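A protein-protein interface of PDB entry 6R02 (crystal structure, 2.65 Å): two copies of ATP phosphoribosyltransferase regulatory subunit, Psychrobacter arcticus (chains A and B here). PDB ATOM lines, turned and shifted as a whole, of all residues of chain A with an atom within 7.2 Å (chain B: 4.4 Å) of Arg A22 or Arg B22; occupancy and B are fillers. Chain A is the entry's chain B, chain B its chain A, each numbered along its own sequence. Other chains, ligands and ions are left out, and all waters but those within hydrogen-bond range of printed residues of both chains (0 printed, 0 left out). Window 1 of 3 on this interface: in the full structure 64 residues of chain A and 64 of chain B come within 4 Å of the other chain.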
ATOM      1  N   ALA A  15      20.534  10.850  27.158  1.00  0.00           N
ATOM      2  CA  ALA A  15      20.216   9.634  26.382  1.00  0.00           C
ATOM      3  C   ALA A  15      18.816   9.141  26.757  1.00  0.00           C
ATOM      4  O   ALA A  15      18.057   8.766  25.845  1.00  0.00           O
ATOM      5  CB  ALA A  15      21.260   8.576  26.621  1.00  0.00           C
ATOM      6  N   HIS A  16      18.492   9.137  28.050  1.00  0.00           N
ATOM      7  CA  HIS A  16      17.152   8.750  28.562  1.00  0.00           C
ATOM      8  C   HIS A  16      16.114   9.703  27.971  1.00  0.00           C
ATOM      9  O   HIS A  16      15.107   9.220  27.422  1.00  0.00           O
ATOM     10  CB  HIS A  16      17.107   8.749  30.097  1.00  0.00           C
ATOM     11  CG  HIS A  16      15.743   8.457  30.634  1.00  0.00           C
ATOM     12  ND1 HIS A  16      15.093   7.259  30.391  1.00  0.00           N
ATOM     13  CD2 HIS A  16      14.894   9.205  31.377  1.00  0.00           C
ATOM     14  CE1 HIS A  16      13.909   7.279  30.976  1.00  0.00           C
ATOM     15  NE2 HIS A  16      13.762   8.462  31.587  1.00  0.00           N
ATOM     16  N   LYS A  17      16.372  11.009  28.072  1.00  0.00           N
ATOM     17  CA  LYS A  17      15.475  12.078  27.563  1.00  0.00           C
ATOM     18  C   LYS A  17      15.232  11.854  26.069  1.00  0.00           C
ATOM     19  O   LYS A  17      14.054  11.753  25.686  1.00  0.00           O
ATOM     20  CB  LYS A  17      16.080  13.460  27.811  1.00  0.00           C
ATOM     21  CG  LYS A  17      15.062  14.563  27.991  1.00  0.00           C
ATOM     22  CD  LYS A  17      15.666  15.944  27.908  1.00  0.00           C
ATOM     23  CE  LYS A  17      16.909  16.121  28.745  1.00  0.00           C
ATOM     24  NZ  LYS A  17      17.135  17.546  29.061  1.00  0.00           N
ATOM     25  N   GLN A  18      16.305  11.754  25.274  1.00  0.00           N
ATOM     26  CA  GLN A  18      16.241  11.526  23.806  1.00  0.00           C
ATOM     27  C   GLN A  18      15.353  10.312  23.520  1.00  0.00           C
ATOM     28  O   GLN A  18      14.500  10.415  22.627  1.00  0.00           O
ATOM     29  CB  GLN A  18      17.635  11.306  23.221  1.00  0.00           C
ATOM     30  CG  GLN A  18      17.647  11.192  21.702  1.00  0.00           C
ATOM     31  CD  GLN A  18      19.042  10.989  21.168  1.00  0.00           C
ATOM     32  OE1 GLN A  18      19.620  11.861  20.522  1.00  0.00           O
ATOM     33  NE2 GLN A  18      19.604   9.830  21.462  1.00  0.00           N
ATOM     34  N   GLU A  19      15.548   9.214  24.254  1.00  0.00           N
ATOM     35  CA  GLU A  19      14.784   7.945  24.089  1.00  0.00           C
ATOM     36  C   GLU A  19      13.297   8.211  24.368  1.00  0.00           C
ATOM     37  O   GLU A  19      12.459   7.706  23.595  1.00  0.00           O
ATOM     38  CB  GLU A  19      15.346   6.860  25.009  1.00  0.00           C
ATOM     39  CG  GLU A  19      14.514   5.589  25.061  1.00  0.00           C
ATOM     40  CD  GLU A  19      14.306   4.925  23.715  1.00  0.00           C
ATOM     41  OE1 GLU A  19      15.277   4.872  22.944  1.00  0.00           O
ATOM     42  OE2 GLU A  19      13.177   4.469  23.435  1.00  0.00           O
ATOM     43  N   VAL A  20      12.981   8.964  25.426  1.00  0.00           N
ATOM     44  CA  VAL A  20      11.570   9.283  25.793  1.00  0.00           C
ATOM     45  C   VAL A  20      10.969  10.164  24.691  1.00  0.00           C
ATOM     46  O   VAL A  20       9.859   9.835  24.219  1.00  0.00           O
ATOM     47  CB  VAL A  20      11.459   9.947  27.179  1.00  0.00           C
ATOM     48  CG1 VAL A  20      10.066  10.516  27.417  1.00  0.00           C
ATOM     49  CG2 VAL A  20      11.829   8.993  28.299  1.00  0.00           C
ATOM     50  N   LEU A  21      11.668  11.234  24.298  1.00  0.00           N
ATOM     51  CA  LEU A  21      11.207  12.165  23.235  1.00  0.00           C
ATOM     52  C   LEU A  21      10.959  11.359  21.957  1.00  0.00           C
ATOM     53  O   LEU A  21       9.832  11.430  21.442  1.00  0.00           O
ATOM     54  CB  LEU A  21      12.240  13.272  22.993  1.00  0.00           C
ATOM     55  CG  LEU A  21      12.454  14.260  24.140  1.00  0.00           C
ATOM     56  CD1 LEU A  21      13.326  15.425  23.708  1.00  0.00           C
ATOM     57  CD2 LEU A  21      11.146  14.777  24.709  1.00  0.00           C
ATOM     58  N   ARG A  22      11.952  10.615  21.470  1.00  0.00           N
ATOM     59  CA  ARG A  22      11.799   9.801  20.237  1.00  0.00           C
ATOM     60  C   ARG A  22      10.481   9.019  20.316  1.00  0.00           C
ATOM     61  O   ARG A  22       9.729   9.032  19.323  1.00  0.00           O
ATOM     62  CB  ARG A  22      12.974   8.846  20.010  1.00  0.00           C
ATOM     63  CG  ARG A  22      12.965   8.231  18.616  1.00  0.00           C
ATOM     64  CD  ARG A  22      13.781   6.954  18.462  1.00  0.00           C
ATOM     65  NE  ARG A  22      13.112   5.776  19.022  1.00  0.00           N
ATOM     66  CZ  ARG A  22      13.562   5.027  20.039  1.00  0.00           C
ATOM     67  NH1 ARG A  22      14.706   5.316  20.637  1.00  0.00           N
ATOM     68  NH2 ARG A  22      12.861   3.986  20.446  1.00  0.00           N
ATOM     69  N   HIS A  23      10.195   8.396  21.463  1.00  0.00           N
ATOM     70  CA  HIS A  23       9.068   7.439  21.624  1.00  0.00           C
ATOM     71  C   HIS A  23       7.739   8.192  21.756  1.00  0.00           C
ATOM     72  O   HIS A  23       6.784   7.800  21.060  1.00  0.00           O
ATOM     73  CB  HIS A  23       9.299   6.482  22.800  1.00  0.00           C
ATOM     74  CG  HIS A  23       8.269   5.404  22.880  1.00  0.00           C
ATOM     75  ND1 HIS A  23       8.181   4.396  21.935  1.00  0.00           N
ATOM     76  CD2 HIS A  23       7.266   5.190  23.762  1.00  0.00           C
ATOM     77  CE1 HIS A  23       7.171   3.602  22.236  1.00  0.00           C
ATOM     78  NE2 HIS A  23       6.590   4.072  23.354  1.00  0.00           N
ATOM     79  N   GLN A  24       7.658   9.191  22.644  1.00  0.00           N
ATOM     80  CA  GLN A  24       6.425   9.998  22.833  1.00  0.00           C
ATOM     81  C   GLN A  24       6.000  10.554  21.471  1.00  0.00           C
ATOM     82  O   GLN A  24       4.846  10.332  21.073  1.00  0.00           O
ATOM     83  CB  GLN A  24       6.632  11.132  23.840  1.00  0.00           C
ATOM     84  CG  GLN A  24       6.379  10.733  25.293  1.00  0.00           C
ATOM     85  CD  GLN A  24       5.297   9.688  25.469  1.00  0.00           C
ATOM     86  OE1 GLN A  24       5.541   8.586  25.968  1.00  0.00           O
ATOM     87  NE2 GLN A  24       4.084  10.028  25.054  1.00  0.00           N
ATOM     88  N   LEU A  25       6.920  11.222  20.775  1.00  0.00           N
ATOM     89  CA  LEU A  25       6.656  11.940  19.498  1.00  0.00           C
ATOM     90  C   LEU A  25       6.256  10.943  18.403  1.00  0.00           C
ATOM     91  O   LEU A  25       5.362  11.265  17.627  1.00  0.00           O
ATOM     92  CB  LEU A  25       7.903  12.739  19.106  1.00  0.00           C
ATOM     93  CG  LEU A  25       8.323  13.836  20.078  1.00  0.00           C
ATOM     94  CD1 LEU A  25       9.655  14.444  19.682  1.00  0.00           C
ATOM     95  CD2 LEU A  25       7.284  14.911  20.170  1.00  0.00           C
ATOM     96  N   THR A  26       6.895   9.775  18.334  1.00  0.00           N
ATOM     97  CA  THR A  26       6.568   8.728  17.333  1.00  0.00           C
ATOM     98  C   THR A  26       5.143   8.227  17.588  1.00  0.00           C
ATOM     99  O   THR A  26       4.388   8.085  16.612  1.00  0.00           O
ATOM    100  CB  THR A  26       7.614   7.606  17.327  1.00  0.00           C
ATOM    101  OG1 THR A  26       8.858   8.184  16.928  1.00  0.00           O
ATOM    102  CG2 THR A  26       7.265   6.474  16.384  1.00  0.00           C
ATOM    103  N   GLN A  27       4.785   7.989  18.854  1.00  0.00           N
ATOM    104  CA  GLN A  27       3.439   7.486  19.244  1.00  0.00           C
ATOM    105  C   GLN A  27       2.389   8.550  18.905  1.00  0.00           C
ATOM    106  O   GLN A  27       1.340   8.173  18.355  1.00  0.00           O
ATOM    107  CB  GLN A  27       3.388   7.081  20.720  1.00  0.00           C
ATOM    108  CG  GLN A  27       4.126   5.786  21.037  1.00  0.00           C
ATOM    109  CD  GLN A  27       3.620   4.618  20.223  1.00  0.00           C
ATOM    110  OE1 GLN A  27       4.385   3.948  19.532  1.00  0.00           O
ATOM    111  NE2 GLN A  27       2.320   4.361  20.285  1.00  0.00           N
ATOM    112  N   GLN A  28       2.665   9.826  19.191  1.00  0.00           N
ATOM    113  CA  GLN A  28       1.758  10.946  18.837  1.00  0.00           C
ATOM    114  C   GLN A  28       1.436  10.877  17.345  1.00  0.00           C
ATOM    115  O   GLN A  28       0.240  10.855  17.014  1.00  0.00           O
ATOM    116  CB  GLN A  28       2.380  12.307  19.152  1.00  0.00           C
ATOM    117  CG  GLN A  28       2.471  12.629  20.629  1.00  0.00           C
ATOM    118  CD  GLN A  28       2.384  14.119  20.840  1.00  0.00           C
ATOM    119  OE1 GLN A  28       3.333  14.771  21.273  1.00  0.00           O
ATOM    120  NE2 GLN A  28       1.251  14.685  20.462  1.00  0.00           N
ATOM    121  N   LEU A  29       2.464  10.831  16.488  1.00  0.00           N
ATOM    122  CA  LEU A  29       2.309  10.840  15.010  1.00  0.00           C
ATOM    123  C   LEU A  29       1.490   9.619  14.579  1.00  0.00           C
ATOM    124  O   LEU A  29       0.625   9.767  13.696  1.00  0.00           O
ATOM    125  CB  LEU A  29       3.688  10.842  14.347  1.00  0.00           C
ATOM    126  CG  LEU A  29       4.490  12.131  14.463  1.00  0.00           C
ATOM    127  CD1 LEU A  29       5.935  11.929  14.044  1.00  0.00           C
ATOM    128  CD2 LEU A  29       3.861  13.204  13.626  1.00  0.00           C
ATOM    129  N   ALA A 100      11.412   8.073  12.409  1.00  0.00           N
ATOM    130  CA  ALA A 100      12.501   8.544  13.285  1.00  0.00           C
ATOM    131  C   ALA A 100      13.704   7.649  13.020  1.00  0.00           C
ATOM    132  O   ALA A 100      13.547   6.418  13.069  1.00  0.00           O
ATOM    133  CB  ALA A 100      12.077   8.506  14.728  1.00  0.00           C
ATOM    134  N   GLY A 101      14.839   8.253  12.691  1.00  0.00           N
ATOM    135  CA  GLY A 101      16.065   7.533  12.320  1.00  0.00           C
ATOM    136  C   GLY A 101      17.260   8.456  12.354  1.00  0.00           C
ATOM    137  O   GLY A 101      17.071   9.682  12.212  1.00  0.00           O
ATOM    138  N   ASP A 102      18.444   7.886  12.560  1.00  0.00           N
ATOM    139  CA  ASP A 102      19.734   8.606  12.429  1.00  0.00           C
ATOM    140  C   ASP A 102      19.972   8.856  10.935  1.00  0.00           C
ATOM    141  O   ASP A 102      19.638   7.982  10.123  1.00  0.00           O
ATOM    142  CB  ASP A 102      20.875   7.833  13.099  1.00  0.00           C
ATOM    143  CG  ASP A 102      20.726   7.683  14.602  1.00  0.00           C
ATOM    144  OD1 ASP A 102      20.559   8.720  15.281  1.00  0.00           O
ATOM    145  OD2 ASP A 102      20.781   6.531  15.083  1.00  0.00           O
ATOM    146  N   LEU A 118      19.174  13.072  14.803  1.00  0.00           N
ATOM    147  CA  LEU A 118      18.091  12.064  14.891  1.00  0.00           C
ATOM    148  C   LEU A 118      16.858  12.665  14.207  1.00  0.00           C
ATOM    149  O   LEU A 118      16.083  13.369  14.876  1.00  0.00           O
ATOM    150  CB  LEU A 118      17.849  11.724  16.364  1.00  0.00           C
ATOM    151  CG  LEU A 118      16.699  10.766  16.655  1.00  0.00           C
ATOM    152  CD1 LEU A 118      16.690   9.587  15.698  1.00  0.00           C
ATOM    153  CD2 LEU A 118      16.779  10.290  18.096  1.00  0.00           C
ATOM    154  N   GLN A 119      16.736  12.443  12.897  1.00  0.00           N
ATOM    155  CA  GLN A 119      15.685  13.043  12.034  1.00  0.00           C
ATOM    156  C   GLN A 119      14.357  12.350  12.343  1.00  0.00           C
ATOM    157  O   GLN A 119      14.286  11.112  12.192  1.00  0.00           O
ATOM    158  CB  GLN A 119      16.048  12.921  10.550  1.00  0.00           C
ATOM    159  CG  GLN A 119      15.054  13.619   9.627  1.00  0.00           C
ATOM    160  CD  GLN A 119      15.468  13.592   8.177  1.00  0.00           C
ATOM    161  OE1 GLN A 119      15.492  12.544   7.529  1.00  0.00           O
ATOM    162  NE2 GLN A 119      15.810  14.755   7.652  1.00  0.00           N
ATOM    163  N   LEU A 120      13.365  13.127  12.782  1.00  0.00           N
ATOM    164  CA  LEU A 120      11.975  12.674  13.046  1.00  0.00           C
ATOM    165  C   LEU A 120      11.026  13.572  12.243  1.00  0.00           C
ATOM    166  O   LEU A 120      11.259  14.805  12.228  1.00  0.00           O
ATOM    167  CB  LEU A 120      11.718  12.764  14.551  1.00  0.00           C
ATOM    168  CG  LEU A 120      10.315  12.376  15.006  1.00  0.00           C
ATOM    169  CD1 LEU A 120      10.338  11.615  16.334  1.00  0.00           C
ATOM    170  CD2 LEU A 120       9.450  13.612  15.128  1.00  0.00           C
ATOM    171  N   VAL A 312      15.602  15.599  16.710  1.00  0.00           N
ATOM    172  CA  VAL A 312      15.130  15.310  18.097  1.00  0.00           C
ATOM    173  C   VAL A 312      16.193  15.793  19.090  1.00  0.00           C
ATOM    174  O   VAL A 312      15.818  16.277  20.157  1.00  0.00           O
ATOM    175  CB  VAL A 312      14.813  13.815  18.305  1.00  0.00           C
ATOM    176  CG1 VAL A 312      14.426  13.517  19.747  1.00  0.00           C
ATOM    177  CG2 VAL A 312      13.709  13.341  17.379  1.00  0.00           C
ATOM    178  N   LEU A 315      16.045  19.223  20.697  1.00  0.00           N
ATOM    179  CA  LEU A 315      15.012  19.388  21.759  1.00  0.00           C
ATOM    180  C   LEU A 315      15.628  19.182  23.146  1.00  0.00           C
ATOM    181  O   LEU A 315      15.071  19.746  24.109  1.00  0.00           O
ATOM    182  CB  LEU A 315      13.875  18.379  21.559  1.00  0.00           C
ATOM    183  CG  LEU A 315      13.008  18.568  20.317  1.00  0.00           C
ATOM    184  CD1 LEU A 315      12.034  17.404  20.165  1.00  0.00           C
ATOM    185  CD2 LEU A 315      12.268  19.892  20.383  1.00  0.00           C
ATOM    186  N   GLN B  18       8.645  -2.904  16.294  1.00  0.00           N
ATOM    187  CA  GLN B  18      10.095  -2.647  16.508  1.00  0.00           C
ATOM    188  C   GLN B  18      10.265  -1.478  17.486  1.00  0.00           C
ATOM    189  O   GLN B  18      11.078  -1.604  18.414  1.00  0.00           O
ATOM    190  CB  GLN B  18      10.794  -2.333  15.187  1.00  0.00           C
ATOM    191  CG  GLN B  18      12.300  -2.167  15.314  1.00  0.00           C
ATOM    192  CD  GLN B  18      12.935  -1.832  13.988  1.00  0.00           C
ATOM    193  OE1 GLN B  18      13.683  -2.625  13.425  1.00  0.00           O
ATOM    194  NE2 GLN B  18      12.625  -0.657  13.466  1.00  0.00           N
ATOM    195  N   GLU B  19       9.519  -0.393  17.283  1.00  0.00           N
ATOM    196  CA  GLU B  19       9.574   0.827  18.131  1.00  0.00           C
ATOM    197  C   GLU B  19       9.149   0.479  19.561  1.00  0.00           C
ATOM    198  O   GLU B  19       9.803   0.953  20.495  1.00  0.00           O
ATOM    199  CB  GLU B  19       8.700   1.934  17.536  1.00  0.00           C
ATOM    200  CG  GLU B  19       8.612   3.175  18.409  1.00  0.00           C
ATOM    201  CD  GLU B  19       9.954   3.797  18.767  1.00  0.00           C
ATOM    202  OE1 GLU B  19      10.842   3.847  17.883  1.00  0.00           O
ATOM    203  OE2 GLU B  19      10.118   4.211  19.937  1.00  0.00           O
ATOM    204  N   VAL B  20       8.094  -0.317  19.728  1.00  0.00           N
ATOM    205  CA  VAL B  20       7.600  -0.743  21.071  1.00  0.00           C
ATOM    206  C   VAL B  20       8.673  -1.618  21.734  1.00  0.00           C
ATOM    207  O   VAL B  20       9.018  -1.344  22.903  1.00  0.00           O
ATOM    208  CB  VAL B  20       6.238  -1.460  20.996  1.00  0.00           C
ATOM    209  CG1 VAL B  20       5.888  -2.145  22.309  1.00  0.00           C
ATOM    210  CG2 VAL B  20       5.120  -0.512  20.579  1.00  0.00           C
ATOM    211  N   LEU B  21       9.182  -2.627  21.021  1.00  0.00           N
ATOM    212  CA  LEU B  21      10.228  -3.538  21.547  1.00  0.00           C
ATOM    213  C   LEU B  21      11.452  -2.720  21.964  1.00  0.00           C
ATOM    214  O   LEU B  21      11.866  -2.839  23.126  1.00  0.00           O
ATOM    215  CB  LEU B  21      10.588  -4.581  20.489  1.00  0.00           C
ATOM    216  CG  LEU B  21       9.499  -5.607  20.180  1.00  0.00           C
ATOM    217  CD1 LEU B  21      10.057  -6.685  19.266  1.00  0.00           C
ATOM    218  CD2 LEU B  21       8.943  -6.227  21.456  1.00  0.00           C
ATOM    219  N   ARG B  22      11.988  -1.893  21.064  1.00  0.00           N
ATOM    220  CA  ARG B  22      13.169  -1.046  21.370  1.00  0.00           C
ATOM    221  C   ARG B  22      12.923  -0.340  22.707  1.00  0.00           C
ATOM    222  O   ARG B  22      13.839  -0.348  23.550  1.00  0.00           O
ATOM    223  CB  ARG B  22      13.454  -0.027  20.261  1.00  0.00           C
ATOM    224  CG  ARG B  22      14.759   0.735  20.441  1.00  0.00           C
ATOM    225  CD  ARG B  22      14.962   1.774  19.368  1.00  0.00           C
ATOM    226  NE  ARG B  22      16.022   2.684  19.763  1.00  0.00           N
ATOM    227  CZ  ARG B  22      16.741   3.436  18.935  1.00  0.00           C
ATOM    228  NH1 ARG B  22      16.519   3.419  17.629  1.00  0.00           N
ATOM    229  NH2 ARG B  22      17.686   4.230  19.415  1.00  0.00           N
ATOM    230  N   HIS B  23      11.725   0.218  22.910  1.00  0.00           N
ATOM    231  CA  HIS B  23      11.413   1.100  24.066  1.00  0.00           C
ATOM    232  C   HIS B  23      11.190   0.272  25.334  1.00  0.00           C
ATOM    233  O   HIS B  23      11.774   0.642  26.363  1.00  0.00           O
ATOM    234  CB  HIS B  23      10.221   2.018  23.771  1.00  0.00           C
ATOM    235  CG  HIS B  23       9.999   3.042  24.833  1.00  0.00           C
ATOM    236  ND1 HIS B  23       8.887   3.024  25.656  1.00  0.00           N
ATOM    237  CD2 HIS B  23      10.747   4.095  25.232  1.00  0.00           C
ATOM    238  CE1 HIS B  23       8.940   4.041  26.491  1.00  0.00           C
ATOM    239  NE2 HIS B  23      10.079   4.707  26.261  1.00  0.00           N
ATOM    240  N   GLN B  24      10.349  -0.770  25.279  1.00  0.00           N
ATOM    241  CA  GLN B  24      10.092  -1.666  26.440  1.00  0.00           C
ATOM    242  C   GLN B  24      11.439  -2.166  26.979  1.00  0.00           C
ATOM    243  O   GLN B  24      11.707  -1.961  28.176  1.00  0.00           O
ATOM    244  CB  GLN B  24       9.194  -2.847  26.066  1.00  0.00           C
ATOM    245  CG  GLN B  24       7.700  -2.562  26.183  1.00  0.00           C
ATOM    246  CD  GLN B  24       6.866  -3.804  25.960  1.00  0.00           C
ATOM    247  OE1 GLN B  24       7.321  -4.928  26.175  1.00  0.00           O
ATOM    248  NE2 GLN B  24       5.627  -3.607  25.531  1.00  0.00           N
ATOM    249  N   LEU B  25      12.260  -2.751  26.104  1.00  0.00           N
ATOM    250  CA  LEU B  25      13.538  -3.415  26.462  1.00  0.00           C
ATOM    251  C   LEU B  25      14.537  -2.384  27.007  1.00  0.00           C
ATOM    252  O   LEU B  25      15.250  -2.721  27.973  1.00  0.00           O
ATOM    253  CB  LEU B  25      14.095  -4.143  25.235  1.00  0.00           C
ATOM    254  CG  LEU B  25      13.213  -5.269  24.693  1.00  0.00           C
ATOM    255  CD1 LEU B  25      13.738  -5.776  23.358  1.00  0.00           C
ATOM    256  CD2 LEU B  25      13.124  -6.415  25.697  1.00  0.00           C
ATOM    257  N   THR B  26      14.603  -1.187  26.423  1.00  0.00           N
ATOM    258  CA  THR B  26      15.516  -0.109  26.887  1.00  0.00           C
ATOM    259  C   THR B  26      15.106   0.304  28.305  1.00  0.00           C
ATOM    260  O   THR B  26      16.005   0.456  29.158  1.00  0.00           O
ATOM    261  CB  THR B  26      15.548   1.080  25.917  1.00  0.00           C
ATOM    262  OG1 THR B  26      16.067   0.608  24.677  1.00  0.00           O
ATOM    263  CG2 THR B  26      16.418   2.222  26.398  1.00  0.00           C
ATOM    264  N   ALA B 100      20.778   1.119  22.585  1.00  0.00           N
ATOM    265  CA  ALA B 100      20.041   0.665  21.392  1.00  0.00           C
ATOM    266  C   ALA B 100      20.379   1.633  20.261  1.00  0.00           C
ATOM    267  O   ALA B 100      20.258   2.850  20.470  1.00  0.00           O
ATOM    268  CB  ALA B 100      18.561   0.599  21.673  1.00  0.00           C
ATOM    269  N   LEU B 118      19.337  -3.596  14.377  1.00  0.00           N
ATOM    270  CA  LEU B 118      19.105  -2.653  15.501  1.00  0.00           C
ATOM    271  C   LEU B 118      19.707  -3.280  16.759  1.00  0.00           C
ATOM    272  O   LEU B 118      19.002  -4.050  17.434  1.00  0.00           O
ATOM    273  CB  LEU B 118      17.600  -2.396  15.623  1.00  0.00           C
ATOM    274  CG  LEU B 118      17.162  -1.510  16.781  1.00  0.00           C
ATOM    275  CD1 LEU B 118      18.060  -0.287  16.932  1.00  0.00           C
ATOM    276  CD2 LEU B 118      15.713  -1.098  16.588  1.00  0.00           C
ATOM    277  N   LEU B 120      20.823  -3.835  20.355  1.00  0.00           N
ATOM    278  CA  LEU B 120      20.427  -3.473  21.740  1.00  0.00           C
ATOM    279  C   LEU B 120      21.197  -4.375  22.707  1.00  0.00           C
ATOM    280  O   LEU B 120      21.296  -5.583  22.417  1.00  0.00           O
ATOM    281  CB  LEU B 120      18.912  -3.655  21.868  1.00  0.00           C
ATOM    282  CG  LEU B 120      18.328  -3.368  23.247  1.00  0.00           C
ATOM    283  CD1 LEU B 120      16.971  -2.702  23.117  1.00  0.00           C
ATOM    284  CD2 LEU B 120      18.214  -4.641  24.075  1.00  0.00           C
ATOM    285  N   VAL B 312      17.238  -6.380  17.626  1.00  0.00           N
ATOM    286  CA  VAL B 312      15.803  -6.183  17.989  1.00  0.00           C
ATOM    287  C   VAL B 312      14.934  -6.654  16.820  1.00  0.00           C
ATOM    288  O   VAL B 312      13.857  -7.213  17.082  1.00  0.00           O
ATOM    289  CB  VAL B 312      15.497  -4.720  18.361  1.00  0.00           C
ATOM    290  CG1 VAL B 312      14.011  -4.506  18.603  1.00  0.00           C
ATOM    291  CG2 VAL B 312      16.305  -4.265  19.574  1.00  0.00           C
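OE2 of Glu B19 lies within hydrogen-bond range of ND1 of His A23. NE2 of His A23 sits close to ND1 of His B23 (3.4 Å). The guanidinium group of Arg B22 is in salt-bridge range of the side-chain carboxylate of Glu A19 (3.9 Å). The side-chain carboxylate (OE2) of Glu B19 is in salt-bridge range of the guanidinium group (NH2) of Arg A22. The guanidinium group (NE) of Arg B22 sits close to the guanidinium group (NH1) of Arg A22 (3.1 Å).
The backbone carbonyl oxygen (O) of Arg A22 sits at hydrogen-bond distance from the side-chain hydroxyl (OG1) of Thr A26 (2.7 Å). The backbone carbonyl oxygen (O) of Arg B22 is in hydrogen-bond range of the side-chain hydroxyl (OG1) of Thr B26 (2.7 Å). The backbone carbonyl oxygen (O) of Ala B100 sits at hydrogen-bond distance from the guanidinium group (NH2) of Arg B22 (3.1 Å). The guanidinium group (NH1) of Arg A22 is in salt-bridge range of the side-chain carboxylate (OE1) of Glu A19 (2.4 Å).
Among the printed residues, merely in contact across the chains: Glu A19 with His B23.
Of chain A, only Glu A19 and Arg A22 come within 4 Å of Arg B22. Of the printed residues of chain B, Glu A19 touches Arg B22 (3.9 Å) and His B23 (3.0 Å). Of the printed residues of chain A, Glu B19 touches Arg A22 (2.8 Å) and His A23 (2.8 Å). Of the printed residues of chain B, His A23 touches Glu B19 (2.8 Å) and His B23 (3.3 Å). Of the printed residues of chain A, His B23 touches Glu A19 (3.0 Å) and His A23 (3.3 Å). Gln A18 touches none of the printed residues of chain B. The nearest residue of chain A that does not touch Arg B22 is Asp A102 (5.8 Å). The nearest printed residue of chain A that does not touch His B23 is Arg A22 (4.6 Å).
Hydrophobic or aromatic side chains of chain A within 4 Å of the printed part of chain B: His A23. Hydrophobic or aromatic side chains of chain B within 4 Å of the printed part of chain A: His B23. Among the printed residues, Asp or Glu carboxylates within 4 Å of a Lys or Arg side-chain nitrogen of the other chain: Glu A19 with Arg B22 and Arg A22 with Glu B19.
Glu A19 touches Arg B22, and with the chains exchanged Arg A22 touches Glu B19. Glu A19 touches His B23, and with the chains exchanged His A23 touches Glu B19. Arg B22 touches its own counterpart, Arg A22. His B23 touches its own counterpart, His A23.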
